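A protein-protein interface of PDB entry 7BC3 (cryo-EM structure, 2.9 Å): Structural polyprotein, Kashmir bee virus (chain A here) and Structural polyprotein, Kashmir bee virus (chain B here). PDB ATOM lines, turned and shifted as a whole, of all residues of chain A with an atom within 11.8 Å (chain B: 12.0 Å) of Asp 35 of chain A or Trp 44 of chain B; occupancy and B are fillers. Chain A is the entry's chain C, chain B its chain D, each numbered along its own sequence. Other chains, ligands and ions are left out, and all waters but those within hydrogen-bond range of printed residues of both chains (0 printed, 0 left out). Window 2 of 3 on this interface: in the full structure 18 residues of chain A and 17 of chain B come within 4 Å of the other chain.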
ATOM      1  N   SER A  29     -26.337  14.838  -9.366  1.00  0.00           N
ATOM      2  CA  SER A  29     -25.223  14.066  -9.894  1.00  0.00           C
ATOM      3  C   SER A  29     -24.090  14.028  -8.879  1.00  0.00           C
ATOM      4  O   SER A  29     -23.675  15.066  -8.358  1.00  0.00           O
ATOM      5  CB  SER A  29     -24.738  14.675 -11.207  1.00  0.00           C
ATOM      6  OG  SER A  29     -25.602  14.338 -12.276  1.00  0.00           O
ATOM      7  N   VAL A  30     -23.592  12.832  -8.601  1.00  0.00           N
ATOM      8  CA  VAL A  30     -22.520  12.673  -7.617  1.00  0.00           C
ATOM      9  C   VAL A  30     -21.186  12.965  -8.294  1.00  0.00           C
ATOM     10  O   VAL A  30     -20.878  12.354  -9.329  1.00  0.00           O
ATOM     11  CB  VAL A  30     -22.538  11.272  -7.025  1.00  0.00           C
ATOM     12  CG1 VAL A  30     -21.348  11.077  -6.114  1.00  0.00           C
ATOM     13  CG2 VAL A  30     -23.826  11.036  -6.269  1.00  0.00           C
ATOM     14  N   PRO A  31     -20.373  13.875  -7.755  1.00  0.00           N
ATOM     15  CA  PRO A  31     -19.076  14.162  -8.373  1.00  0.00           C
ATOM     16  C   PRO A  31     -17.992  13.190  -7.936  1.00  0.00           C
ATOM     17  O   PRO A  31     -17.794  12.923  -6.750  1.00  0.00           O
ATOM     18  CB  PRO A  31     -18.776  15.582  -7.880  1.00  0.00           C
ATOM     19  CG  PRO A  31     -19.440  15.662  -6.565  1.00  0.00           C
ATOM     20  CD  PRO A  31     -20.644  14.766  -6.614  1.00  0.00           C
ATOM     21  N   LEU A  32     -17.282  12.658  -8.926  1.00  0.00           N
ATOM     22  CA  LEU A  32     -16.158  11.756  -8.680  1.00  0.00           C
ATOM     23  C   LEU A  32     -14.902  12.566  -8.369  1.00  0.00           C
ATOM     24  O   LEU A  32     -13.865  12.452  -9.018  1.00  0.00           O
ATOM     25  CB  LEU A  32     -15.939  10.846  -9.879  1.00  0.00           C
ATOM     26  CG  LEU A  32     -17.164  10.063 -10.326  1.00  0.00           C
ATOM     27  CD1 LEU A  32     -16.888   9.372 -11.636  1.00  0.00           C
ATOM     28  CD2 LEU A  32     -17.543   9.070  -9.259  1.00  0.00           C
ATOM     29  N   ALA A  33     -15.021  13.398  -7.344  1.00  0.00           N
ATOM     30  CA  ALA A  33     -14.013  14.390  -7.024  1.00  0.00           C
ATOM     31  C   ALA A  33     -13.598  14.252  -5.568  1.00  0.00           C
ATOM     32  O   ALA A  33     -13.980  13.314  -4.864  1.00  0.00           O
ATOM     33  CB  ALA A  33     -14.533  15.804  -7.300  1.00  0.00           C
ATOM     34  N   TYR A  34     -12.795  15.215  -5.134  1.00  0.00           N
ATOM     35  CA  TYR A  34     -12.388  15.368  -3.750  1.00  0.00           C
ATOM     36  C   TYR A  34     -13.281  16.354  -3.009  1.00  0.00           C
ATOM     37  O   TYR A  34     -13.843  15.999  -1.971  1.00  0.00           O
ATOM     38  CB  TYR A  34     -10.909  15.795  -3.737  1.00  0.00           C
ATOM     39  CG  TYR A  34     -10.286  16.318  -2.464  1.00  0.00           C
ATOM     40  CD1 TYR A  34      -9.869  15.456  -1.461  1.00  0.00           C
ATOM     41  CD2 TYR A  34     -10.014  17.670  -2.316  1.00  0.00           C
ATOM     42  CE1 TYR A  34      -9.263  15.935  -0.316  1.00  0.00           C
ATOM     43  CE2 TYR A  34      -9.412  18.157  -1.175  1.00  0.00           C
ATOM     44  CZ  TYR A  34      -9.038  17.287  -0.180  1.00  0.00           C
ATOM     45  OH  TYR A  34      -8.433  17.771   0.954  1.00  0.00           O
ATOM     46  N   ASP A  35     -13.530  17.527  -3.586  1.00  0.00           N
ATOM     47  CA  ASP A  35     -14.348  18.574  -2.997  1.00  0.00           C
ATOM     48  C   ASP A  35     -15.752  18.565  -3.591  1.00  0.00           C
ATOM     49  O   ASP A  35     -15.895  18.491  -4.819  1.00  0.00           O
ATOM     50  CB  ASP A  35     -13.689  19.945  -3.235  1.00  0.00           C
ATOM     51  CG  ASP A  35     -14.215  21.025  -2.314  1.00  0.00           C
ATOM     52  OD1 ASP A  35     -15.408  20.985  -1.957  1.00  0.00           O
ATOM     53  OD2 ASP A  35     -13.430  21.923  -1.946  1.00  0.00           O
ATOM     54  N   PRO A  36     -16.809  18.633  -2.771  1.00  0.00           N
ATOM     55  CA  PRO A  36     -18.147  18.824  -3.349  1.00  0.00           C
ATOM     56  C   PRO A  36     -18.303  20.175  -4.011  1.00  0.00           C
ATOM     57  O   PRO A  36     -19.104  20.313  -4.944  1.00  0.00           O
ATOM     58  CB  PRO A  36     -19.090  18.682  -2.145  1.00  0.00           C
ATOM     59  CG  PRO A  36     -18.260  18.198  -1.018  1.00  0.00           C
ATOM     60  CD  PRO A  36     -16.859  18.581  -1.300  1.00  0.00           C
ATOM     61  N   ASN A  37     -17.557  21.177  -3.553  1.00  0.00           N
ATOM     62  CA  ASN A  37     -17.585  22.510  -4.128  1.00  0.00           C
ATOM     63  C   ASN A  37     -16.586  22.668  -5.265  1.00  0.00           C
ATOM     64  O   ASN A  37     -16.162  23.790  -5.560  1.00  0.00           O
ATOM     65  CB  ASN A  37     -17.327  23.547  -3.037  1.00  0.00           C
ATOM     66  CG  ASN A  37     -18.492  23.681  -2.082  1.00  0.00           C
ATOM     67  OD1 ASN A  37     -18.472  23.139  -0.978  1.00  0.00           O
ATOM     68  ND2 ASN A  37     -19.523  24.401  -2.508  1.00  0.00           N
ATOM     69  N   ASN A  38     -16.196  21.564  -5.897  1.00  0.00           N
ATOM     70  CA  ASN A  38     -15.382  21.625  -7.100  1.00  0.00           C
ATOM     71  C   ASN A  38     -16.028  22.540  -8.128  1.00  0.00           C
ATOM     72  O   ASN A  38     -17.211  22.398  -8.452  1.00  0.00           O
ATOM     73  CB  ASN A  38     -15.210  20.218  -7.675  1.00  0.00           C
ATOM     74  CG  ASN A  38     -14.467  20.211  -8.992  1.00  0.00           C
ATOM     75  OD1 ASN A  38     -14.956  20.721 -10.001  1.00  0.00           O
ATOM     76  ND2 ASN A  38     -13.284  19.618  -8.995  1.00  0.00           N
ATOM     77  N   GLU A  39     -15.244  23.484  -8.640  1.00  0.00           N
ATOM     78  CA  GLU A  39     -15.736  24.421  -9.639  1.00  0.00           C
ATOM     79  C   GLU A  39     -14.542  25.031 -10.352  1.00  0.00           C
ATOM     80  O   GLU A  39     -13.602  25.494  -9.700  1.00  0.00           O
ATOM     81  CB  GLU A  39     -16.596  25.516  -8.998  1.00  0.00           C
ATOM     82  CG  GLU A  39     -15.826  26.456  -8.092  1.00  0.00           C
ATOM     83  CD  GLU A  39     -16.663  26.974  -6.941  1.00  0.00           C
ATOM     84  OE1 GLU A  39     -16.592  26.386  -5.841  1.00  0.00           O
ATOM     85  OE2 GLU A  39     -17.391  27.969  -7.135  1.00  0.00           O
ATOM     86  N   LEU A  40     -14.577  25.020 -11.679  1.00  0.00           N
ATOM     87  CA  LEU A  40     -13.537  25.685 -12.440  1.00  0.00           C
ATOM     88  C   LEU A  40     -13.645  27.194 -12.256  1.00  0.00           C
ATOM     89  O   LEU A  40     -14.636  27.718 -11.740  1.00  0.00           O
ATOM     90  CB  LEU A  40     -13.643  25.336 -13.924  1.00  0.00           C
ATOM     91  CG  LEU A  40     -13.121  23.978 -14.397  1.00  0.00           C
ATOM     92  CD1 LEU A  40     -11.629  23.898 -14.205  1.00  0.00           C
ATOM     93  CD2 LEU A  40     -13.814  22.836 -13.680  1.00  0.00           C
ATOM     94  N   GLY A  41     -12.606  27.897 -12.689  1.00  0.00           N
ATOM     95  CA  GLY A  41     -12.598  29.340 -12.645  1.00  0.00           C
ATOM     96  C   GLY A  41     -13.292  29.936 -13.852  1.00  0.00           C
ATOM     97  O   GLY A  41     -13.919  29.249 -14.659  1.00  0.00           O
ATOM     98  N   ASP A  42     -13.173  31.254 -13.969  1.00  0.00           N
ATOM     99  CA  ASP A  42     -13.725  31.937 -15.123  1.00  0.00           C
ATOM    100  C   ASP A  42     -12.834  31.708 -16.344  1.00  0.00           C
ATOM    101  O   ASP A  42     -11.772  31.083 -16.271  1.00  0.00           O
ATOM    102  CB  ASP A  42     -13.890  33.428 -14.837  1.00  0.00           C
ATOM    103  CG  ASP A  42     -12.570  34.121 -14.563  1.00  0.00           C
ATOM    104  OD1 ASP A  42     -11.678  33.486 -13.967  1.00  0.00           O
ATOM    105  OD2 ASP A  42     -12.429  35.301 -14.946  1.00  0.00           O
ATOM    106  N   ALA B  35     -18.514  36.345 -11.982  1.00  0.00           N
ATOM    107  CA  ALA B  35     -17.294  36.676 -11.252  1.00  0.00           C
ATOM    108  C   ALA B  35     -16.799  35.405 -10.572  1.00  0.00           C
ATOM    109  O   ALA B  35     -17.340  34.991  -9.544  1.00  0.00           O
ATOM    110  CB  ALA B  35     -17.554  37.783 -10.234  1.00  0.00           C
ATOM    111  N   LYS B  36     -15.772  34.789 -11.149  1.00  0.00           N
ATOM    112  CA  LYS B  36     -15.122  33.641 -10.536  1.00  0.00           C
ATOM    113  C   LYS B  36     -13.615  33.742 -10.737  1.00  0.00           C
ATOM    114  O   LYS B  36     -12.988  32.798 -11.234  1.00  0.00           O
ATOM    115  CB  LYS B  36     -15.658  32.336 -11.126  1.00  0.00           C
ATOM    116  CG  LYS B  36     -16.951  31.852 -10.498  1.00  0.00           C
ATOM    117  CD  LYS B  36     -17.124  30.351 -10.661  1.00  0.00           C
ATOM    118  CE  LYS B  36     -17.401  29.979 -12.109  1.00  0.00           C
ATOM    119  NZ  LYS B  36     -17.229  28.522 -12.355  1.00  0.00           N
ATOM    120  N   PRO B  37     -12.998  34.864 -10.367  1.00  0.00           N
ATOM    121  CA  PRO B  37     -11.544  34.986 -10.513  1.00  0.00           C
ATOM    122  C   PRO B  37     -10.805  34.233  -9.422  1.00  0.00           C
ATOM    123  O   PRO B  37     -11.422  33.492  -8.649  1.00  0.00           O
ATOM    124  CB  PRO B  37     -11.317  36.497 -10.416  1.00  0.00           C
ATOM    125  CG  PRO B  37     -12.387  36.957  -9.504  1.00  0.00           C
ATOM    126  CD  PRO B  37     -13.580  36.060  -9.734  1.00  0.00           C
ATOM    127  N   VAL B  38      -9.489  34.412  -9.341  1.00  0.00           N
ATOM    128  CA  VAL B  38      -8.714  33.776  -8.287  1.00  0.00           C
ATOM    129  C   VAL B  38      -8.841  34.643  -7.045  1.00  0.00           C
ATOM    130  O   VAL B  38      -7.987  35.493  -6.770  1.00  0.00           O
ATOM    131  CB  VAL B  38      -7.241  33.594  -8.698  1.00  0.00           C
ATOM    132  CG1 VAL B  38      -6.496  32.765  -7.665  1.00  0.00           C
ATOM    133  CG2 VAL B  38      -7.143  32.951 -10.074  1.00  0.00           C
ATOM    134  N   THR B  39      -9.912  34.423  -6.287  1.00  0.00           N
ATOM    135  CA  THR B  39     -10.242  35.240  -5.130  1.00  0.00           C
ATOM    136  C   THR B  39     -11.014  34.374  -4.142  1.00  0.00           C
ATOM    137  O   THR B  39     -11.213  33.176  -4.364  1.00  0.00           O
ATOM    138  CB  THR B  39     -11.066  36.468  -5.538  1.00  0.00           C
ATOM    139  OG1 THR B  39     -12.147  36.058  -6.382  1.00  0.00           O
ATOM    140  CG2 THR B  39     -10.216  37.484  -6.272  1.00  0.00           C
ATOM    141  N   ALA B  40     -11.468  34.992  -3.053  1.00  0.00           N
ATOM    142  CA  ALA B  40     -12.379  34.326  -2.134  1.00  0.00           C
ATOM    143  C   ALA B  40     -13.776  34.154  -2.714  1.00  0.00           C
ATOM    144  O   ALA B  40     -14.653  33.630  -2.019  1.00  0.00           O
ATOM    145  CB  ALA B  40     -12.454  35.105  -0.823  1.00  0.00           C
ATOM    146  N   ALA B  41     -14.005  34.582  -3.958  1.00  0.00           N
ATOM    147  CA  ALA B  41     -15.284  34.341  -4.611  1.00  0.00           C
ATOM    148  C   ALA B  41     -15.523  32.864  -4.873  1.00  0.00           C
ATOM    149  O   ALA B  41     -16.680  32.444  -4.981  1.00  0.00           O
ATOM    150  CB  ALA B  41     -15.355  35.110  -5.928  1.00  0.00           C
ATOM    151  N   VAL B  42     -14.466  32.078  -4.985  1.00  0.00           N
ATOM    152  CA  VAL B  42     -14.573  30.640  -5.182  1.00  0.00           C
ATOM    153  C   VAL B  42     -14.538  29.967  -3.818  1.00  0.00           C
ATOM    154  O   VAL B  42     -13.780  30.370  -2.928  1.00  0.00           O
ATOM    155  CB  VAL B  42     -13.448  30.130  -6.098  1.00  0.00           C
ATOM    156  CG1 VAL B  42     -13.676  28.683  -6.466  1.00  0.00           C
ATOM    157  CG2 VAL B  42     -13.373  30.985  -7.348  1.00  0.00           C
ATOM    158  N   LYS B  43     -15.362  28.934  -3.655  1.00  0.00           N
ATOM    159  CA  LYS B  43     -15.574  28.361  -2.331  1.00  0.00           C
ATOM    160  C   LYS B  43     -14.306  27.706  -1.799  1.00  0.00           C
ATOM    161  O   LYS B  43     -13.865  28.005  -0.684  1.00  0.00           O
ATOM    162  CB  LYS B  43     -16.722  27.356  -2.383  1.00  0.00           C
ATOM    163  CG  LYS B  43     -17.001  26.657  -1.067  1.00  0.00           C
ATOM    164  CD  LYS B  43     -17.469  27.626  -0.010  1.00  0.00           C
ATOM    165  CE  LYS B  43     -17.872  26.898   1.254  1.00  0.00           C
ATOM    166  NZ  LYS B  43     -16.703  26.607   2.119  1.00  0.00           N
ATOM    167  N   TRP B  44     -13.709  26.802  -2.575  1.00  0.00           N
ATOM    168  CA  TRP B  44     -12.536  26.087  -2.083  1.00  0.00           C
ATOM    169  C   TRP B  44     -11.340  27.019  -1.932  1.00  0.00           C
ATOM    170  O   TRP B  44     -10.541  26.866  -1.001  1.00  0.00           O
ATOM    171  CB  TRP B  44     -12.202  24.916  -3.007  1.00  0.00           C
ATOM    172  CG  TRP B  44     -12.053  25.275  -4.448  1.00  0.00           C
ATOM    173  CD1 TRP B  44     -13.039  25.320  -5.385  1.00  0.00           C
ATOM    174  CD2 TRP B  44     -10.841  25.619  -5.124  1.00  0.00           C
ATOM    175  NE1 TRP B  44     -12.519  25.680  -6.602  1.00  0.00           N
ATOM    176  CE2 TRP B  44     -11.170  25.869  -6.468  1.00  0.00           C
ATOM    177  CE3 TRP B  44      -9.509  25.745  -4.722  1.00  0.00           C
ATOM    178  CZ2 TRP B  44     -10.219  26.236  -7.411  1.00  0.00           C
ATOM    179  CZ3 TRP B  44      -8.568  26.110  -5.660  1.00  0.00           C
ATOM    180  CH2 TRP B  44      -8.926  26.352  -6.988  1.00  0.00           C
ATOM    181  N   PHE B  45     -11.206  28.005  -2.818  1.00  0.00           N
ATOM    182  CA  PHE B  45     -10.096  28.941  -2.696  1.00  0.00           C
ATOM    183  C   PHE B  45     -10.251  29.816  -1.459  1.00  0.00           C
ATOM    184  O   PHE B  45      -9.264  30.115  -0.772  1.00  0.00           O
ATOM    185  CB  PHE B  45      -9.996  29.803  -3.950  1.00  0.00           C
ATOM    186  CG  PHE B  45      -8.718  30.575  -4.047  1.00  0.00           C
ATOM    187  CD1 PHE B  45      -7.569  29.976  -4.525  1.00  0.00           C
ATOM    188  CD2 PHE B  45      -8.663  31.897  -3.650  1.00  0.00           C
ATOM    189  CE1 PHE B  45      -6.393  30.682  -4.611  1.00  0.00           C
ATOM    190  CE2 PHE B  45      -7.489  32.607  -3.733  1.00  0.00           C
ATOM    191  CZ  PHE B  45      -6.353  32.000  -4.214  1.00  0.00           C
ATOM    192  N   ALA B  46     -11.478  30.250  -1.173  1.00  0.00           N
ATOM    193  CA  ALA B  46     -11.736  30.966   0.070  1.00  0.00           C
ATOM    194  C   ALA B  46     -11.446  30.082   1.272  1.00  0.00           C
ATOM    195  O   ALA B  46     -10.873  30.539   2.266  1.00  0.00           O
ATOM    196  CB  ALA B  46     -13.183  31.454   0.099  1.00  0.00           C
ATOM    197  N   ASP B  47     -11.833  28.810   1.195  1.00  0.00           N
ATOM    198  CA  ASP B  47     -11.524  27.867   2.262  1.00  0.00           C
ATOM    199  C   ASP B  47     -10.025  27.804   2.516  1.00  0.00           C
ATOM    200  O   ASP B  47      -9.582  27.788   3.669  1.00  0.00           O
ATOM    201  CB  ASP B  47     -12.056  26.487   1.890  1.00  0.00           C
ATOM    202  CG  ASP B  47     -13.541  26.343   2.139  1.00  0.00           C
ATOM    203  OD1 ASP B  47     -14.277  27.332   1.957  1.00  0.00           O
ATOM    204  OD2 ASP B  47     -13.972  25.227   2.494  1.00  0.00           O
ATOM    205  N   ILE B  48      -9.231  27.769   1.448  1.00  0.00           N
ATOM    206  CA  ILE B  48      -7.784  27.663   1.599  1.00  0.00           C
ATOM    207  C   ILE B  48      -7.217  28.943   2.199  1.00  0.00           C
ATOM    208  O   ILE B  48      -6.609  28.931   3.275  1.00  0.00           O
ATOM    209  CB  ILE B  48      -7.116  27.348   0.251  1.00  0.00           C
ATOM    210  CG1 ILE B  48      -7.676  26.055  -0.347  1.00  0.00           C
ATOM    211  CG2 ILE B  48      -5.611  27.245   0.428  1.00  0.00           C
ATOM    212  CD1 ILE B  48      -7.063  24.805   0.204  1.00  0.00           C
ATOM    213  N   VAL B  49      -7.404  30.068   1.504  1.00  0.00           N
ATOM    214  CA  VAL B  49      -6.756  31.310   1.912  1.00  0.00           C
ATOM    215  C   VAL B  49      -7.305  31.868   3.213  1.00  0.00           C
ATOM    216  O   VAL B  49      -6.637  32.688   3.852  1.00  0.00           O
ATOM    217  CB  VAL B  49      -6.873  32.372   0.803  1.00  0.00           C
ATOM    218  CG1 VAL B  49      -6.299  31.835  -0.494  1.00  0.00           C
ATOM    219  CG2 VAL B  49      -8.315  32.798   0.624  1.00  0.00           C
ATOM    220  N   GLY B  50      -8.498  31.452   3.624  1.00  0.00           N
ATOM    221  CA  GLY B  50      -9.015  31.786   4.928  1.00  0.00           C
ATOM    222  C   GLY B  50      -8.619  30.808   6.002  1.00  0.00           C
ATOM    223  O   GLY B  50      -8.974  30.998   7.169  1.00  0.00           O
ATOM    224  N   GLY B  51      -7.882  29.764   5.637  1.00  0.00           N
ATOM    225  CA  GLY B  51      -7.484  28.751   6.596  1.00  0.00           C
ATOM    226  C   GLY B  51      -8.632  28.235   7.431  1.00  0.00           C
ATOM    227  O   GLY B  51      -8.670  28.474   8.643  1.00  0.00           O
ATOM    228  N   VAL B  52      -9.597  27.559   6.804  1.00  0.00           N
ATOM    229  CA  VAL B  52     -10.629  26.902   7.587  1.00  0.00           C
ATOM    230  C   VAL B  52     -10.101  25.556   8.077  1.00  0.00           C
ATOM    231  O   VAL B  52      -9.113  25.015   7.567  1.00  0.00           O
ATOM    232  CB  VAL B  52     -11.931  26.728   6.789  1.00  0.00           C
ATOM    233  CG1 VAL B  52     -12.492  28.082   6.403  1.00  0.00           C
ATOM    234  CG2 VAL B  52     -11.708  25.867   5.562  1.00  0.00           C
ATOM    235  N   ALA B  53     -10.772  25.015   9.090  1.00  0.00           N
ATOM    236  CA  ALA B  53     -10.316  23.791   9.731  1.00  0.00           C
ATOM    237  C   ALA B  53     -10.661  22.537   8.942  1.00  0.00           C
ATOM    238  O   ALA B  53     -10.225  21.447   9.328  1.00  0.00           O
ATOM    239  CB  ALA B  53     -10.912  23.691  11.134  1.00  0.00           C
ATOM    240  N   ALA B  54     -11.420  22.657   7.854  1.00  0.00           N
ATOM    241  CA  ALA B  54     -11.825  21.479   7.101  1.00  0.00           C
ATOM    242  C   ALA B  54     -10.757  21.038   6.111  1.00  0.00           C
ATOM    243  O   ALA B  54     -10.607  19.837   5.864  1.00  0.00           O
ATOM    244  CB  ALA B  54     -13.135  21.752   6.368  1.00  0.00           C
ATOM    245  N   ILE B  55     -10.009  21.983   5.538  1.00  0.00           N
ATOM    246  CA  ILE B  55      -8.924  21.633   4.631  1.00  0.00           C
ATOM    247  C   ILE B  55      -7.819  20.859   5.326  1.00  0.00           C
ATOM    248  O   ILE B  55      -6.954  20.287   4.653  1.00  0.00           O
ATOM    249  CB  ILE B  55      -8.341  22.901   3.974  1.00  0.00           C
ATOM    250  CG1 ILE B  55      -7.874  23.895   5.035  1.00  0.00           C
ATOM    251  CG2 ILE B  55      -9.374  23.558   3.085  1.00  0.00           C
ATOM    252  CD1 ILE B  55      -6.768  24.797   4.564  1.00  0.00           C
ATOM    253  N   PHE B  56      -7.826  20.830   6.657  1.00  0.00           N
ATOM    254  CA  PHE B  56      -6.881  20.051   7.438  1.00  0.00           C
ATOM    255  C   PHE B  56      -7.463  18.729   7.914  1.00  0.00           C
ATOM    256  O   PHE B  56      -6.732  17.916   8.483  1.00  0.00           O
ATOM    257  CB  PHE B  56      -6.408  20.861   8.647  1.00  0.00           C
ATOM    258  CG  PHE B  56      -5.785  22.175   8.291  1.00  0.00           C
ATOM    259  CD1 PHE B  56      -4.615  22.224   7.558  1.00  0.00           C
ATOM    260  CD2 PHE B  56      -6.364  23.363   8.695  1.00  0.00           C
ATOM    261  CE1 PHE B  56      -4.039  23.429   7.232  1.00  0.00           C
ATOM    262  CE2 PHE B  56      -5.790  24.571   8.371  1.00  0.00           C
ATOM    263  CZ  PHE B  56      -4.626  24.605   7.639  1.00  0.00           C
ATOM    264  N   GLY B  57      -8.754  18.502   7.703  1.00  0.00           N
ATOM    265  CA  GLY B  57      -9.397  17.281   8.127  1.00  0.00           C
ATOM    266  C   GLY B  57     -10.151  17.372   9.433  1.00  0.00           C
ATOM    267  O   GLY B  57     -10.555  16.332   9.963  1.00  0.00           O
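Asp 35 of chain A touches just one residue of chain B: Trp 44 (3.4 Å). Printed residues of chain A within 4 Å of Trp 44 of chain B: Asp 35, Asn 37 and Glu 39. Pro 31 of chain A touches none of the printed residues of chain B. No residue of chain B comes within 4 Å of Tyr 34 of chain A. No residue of chain B comes within 4 Å of Pro 36 of chain A. Of chain B, only Lys 43 (3.5 Å) and Trp 44 (3.5 Å) come within 4 Å of Asn 37 of chain A. Of chain B, only Val 42 (3.5 Å), Lys 43 (3.6 Å) and Trp 44 (3.3 Å) come within 4 Å of Glu 39 of chain A. Leu 40 of chain A touches just one residue of chain B: Lys 36. Of chain A, only Glu 39 (3.5 Å) comes within 4 Å of Val 42 of chain B. Of chain A, only Asn 37 (3.5 Å) and Glu 39 (3.6 Å) come within 4 Å of Lys 43 of chain B. No residue of chain A comes within 4 Å of Asp 47 of chain B. No residue of chain A comes within 4 Å of Ile 48 of chain B. Printed residues of chain B within 4 Å of Gly 41 of chain A: Lys 36. Printed residues of chain A within 4 Å of Lys 36 of chain B: Leu 40, Gly 41 and Asp 42. Printed residues of chain A within 4 Å of Pro 37 of chain B: Asp 42 (3.8 Å). Of the printed residues of chain B, Asp 42 of chain A touches Lys 36 (3.1 Å) and Pro 37 (3.8 Å). Thr 39 of chain B touches none of the printed residues of chain A. Val 52 of chain B touches none of the printed residues of chain A. The nearest residue of chain B that does not touch Asp 35 of chain A is Asp 47 of chain B (5.6 Å).
Asp 35 of chain A touches Trp 44 of chain B (OD2 to CB, 3.4 Å). Lys 43 of chain B touches Asn 37 of chain A. O of Asn 37 of chain A touches CD1 of Trp 44 of chain B (3.5 Å). Glu 39 of chain A touches Val 42 of chain B. Lys 43 of chain B touches Glu 39 of chain A (N to OE1, 3.6 Å). CA of Gly 41 of chain A touches O of Lys 36 of chain B (3.8 Å). Asp 42 of chain A touches Pro 37 of chain B.
The backbone carbonyl oxygen (O) of Leu 40 of chain A sits at hydrogen-bond distance from the side-chain amino group (NZ) of Lys 36 of chain B. N of Asp 42 of chain A is in hydrogen-bond range of O of Lys 36 of chain B (3.1 Å). NE1 of Trp 44 of chain B sits at hydrogen-bond distance from O of Glu 39 of chain A (3.3 Å).
The backbone carbonyl oxygen of Pro 37 of chain B sits close to the side-chain hydroxyl of Thr 39 of chain B, 3.5 Å away. NZ of Lys 43 of chain B is in salt-bridge range of OD1 of Asp 47 of chain B. OD1 of Asp 35 of chain A sits at hydrogen-bond distance from N of Asn 37 of chain A (2.7 Å). The side-chain carboxylate of Glu 39 of chain A sits close to the backbone carbonyl oxygen of Asn 37 of chain A (2.6 Å).
Printed residues of chain B that touch a printed residue of chain A: Lys 36, Pro 37, Val 42, Lys 43 and Trp 44. Hydrophobic or aromatic side chains of chain B that line the printed part of chain A: Val 42 and Trp 44. Along chain B the printed residues that touch a printed residue of chain A span positions 36 to 44. Of the 14 printed residues of chain A, 6 touch a printed residue of chain B. Along chain A the printed residues that touch a printed residue of chain B span positions 35 to 42. Among the printed residues, no Asp or Glu carboxylate lies within 4 Å of a Lys or Arg side-chain nitrogen of the other chain.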
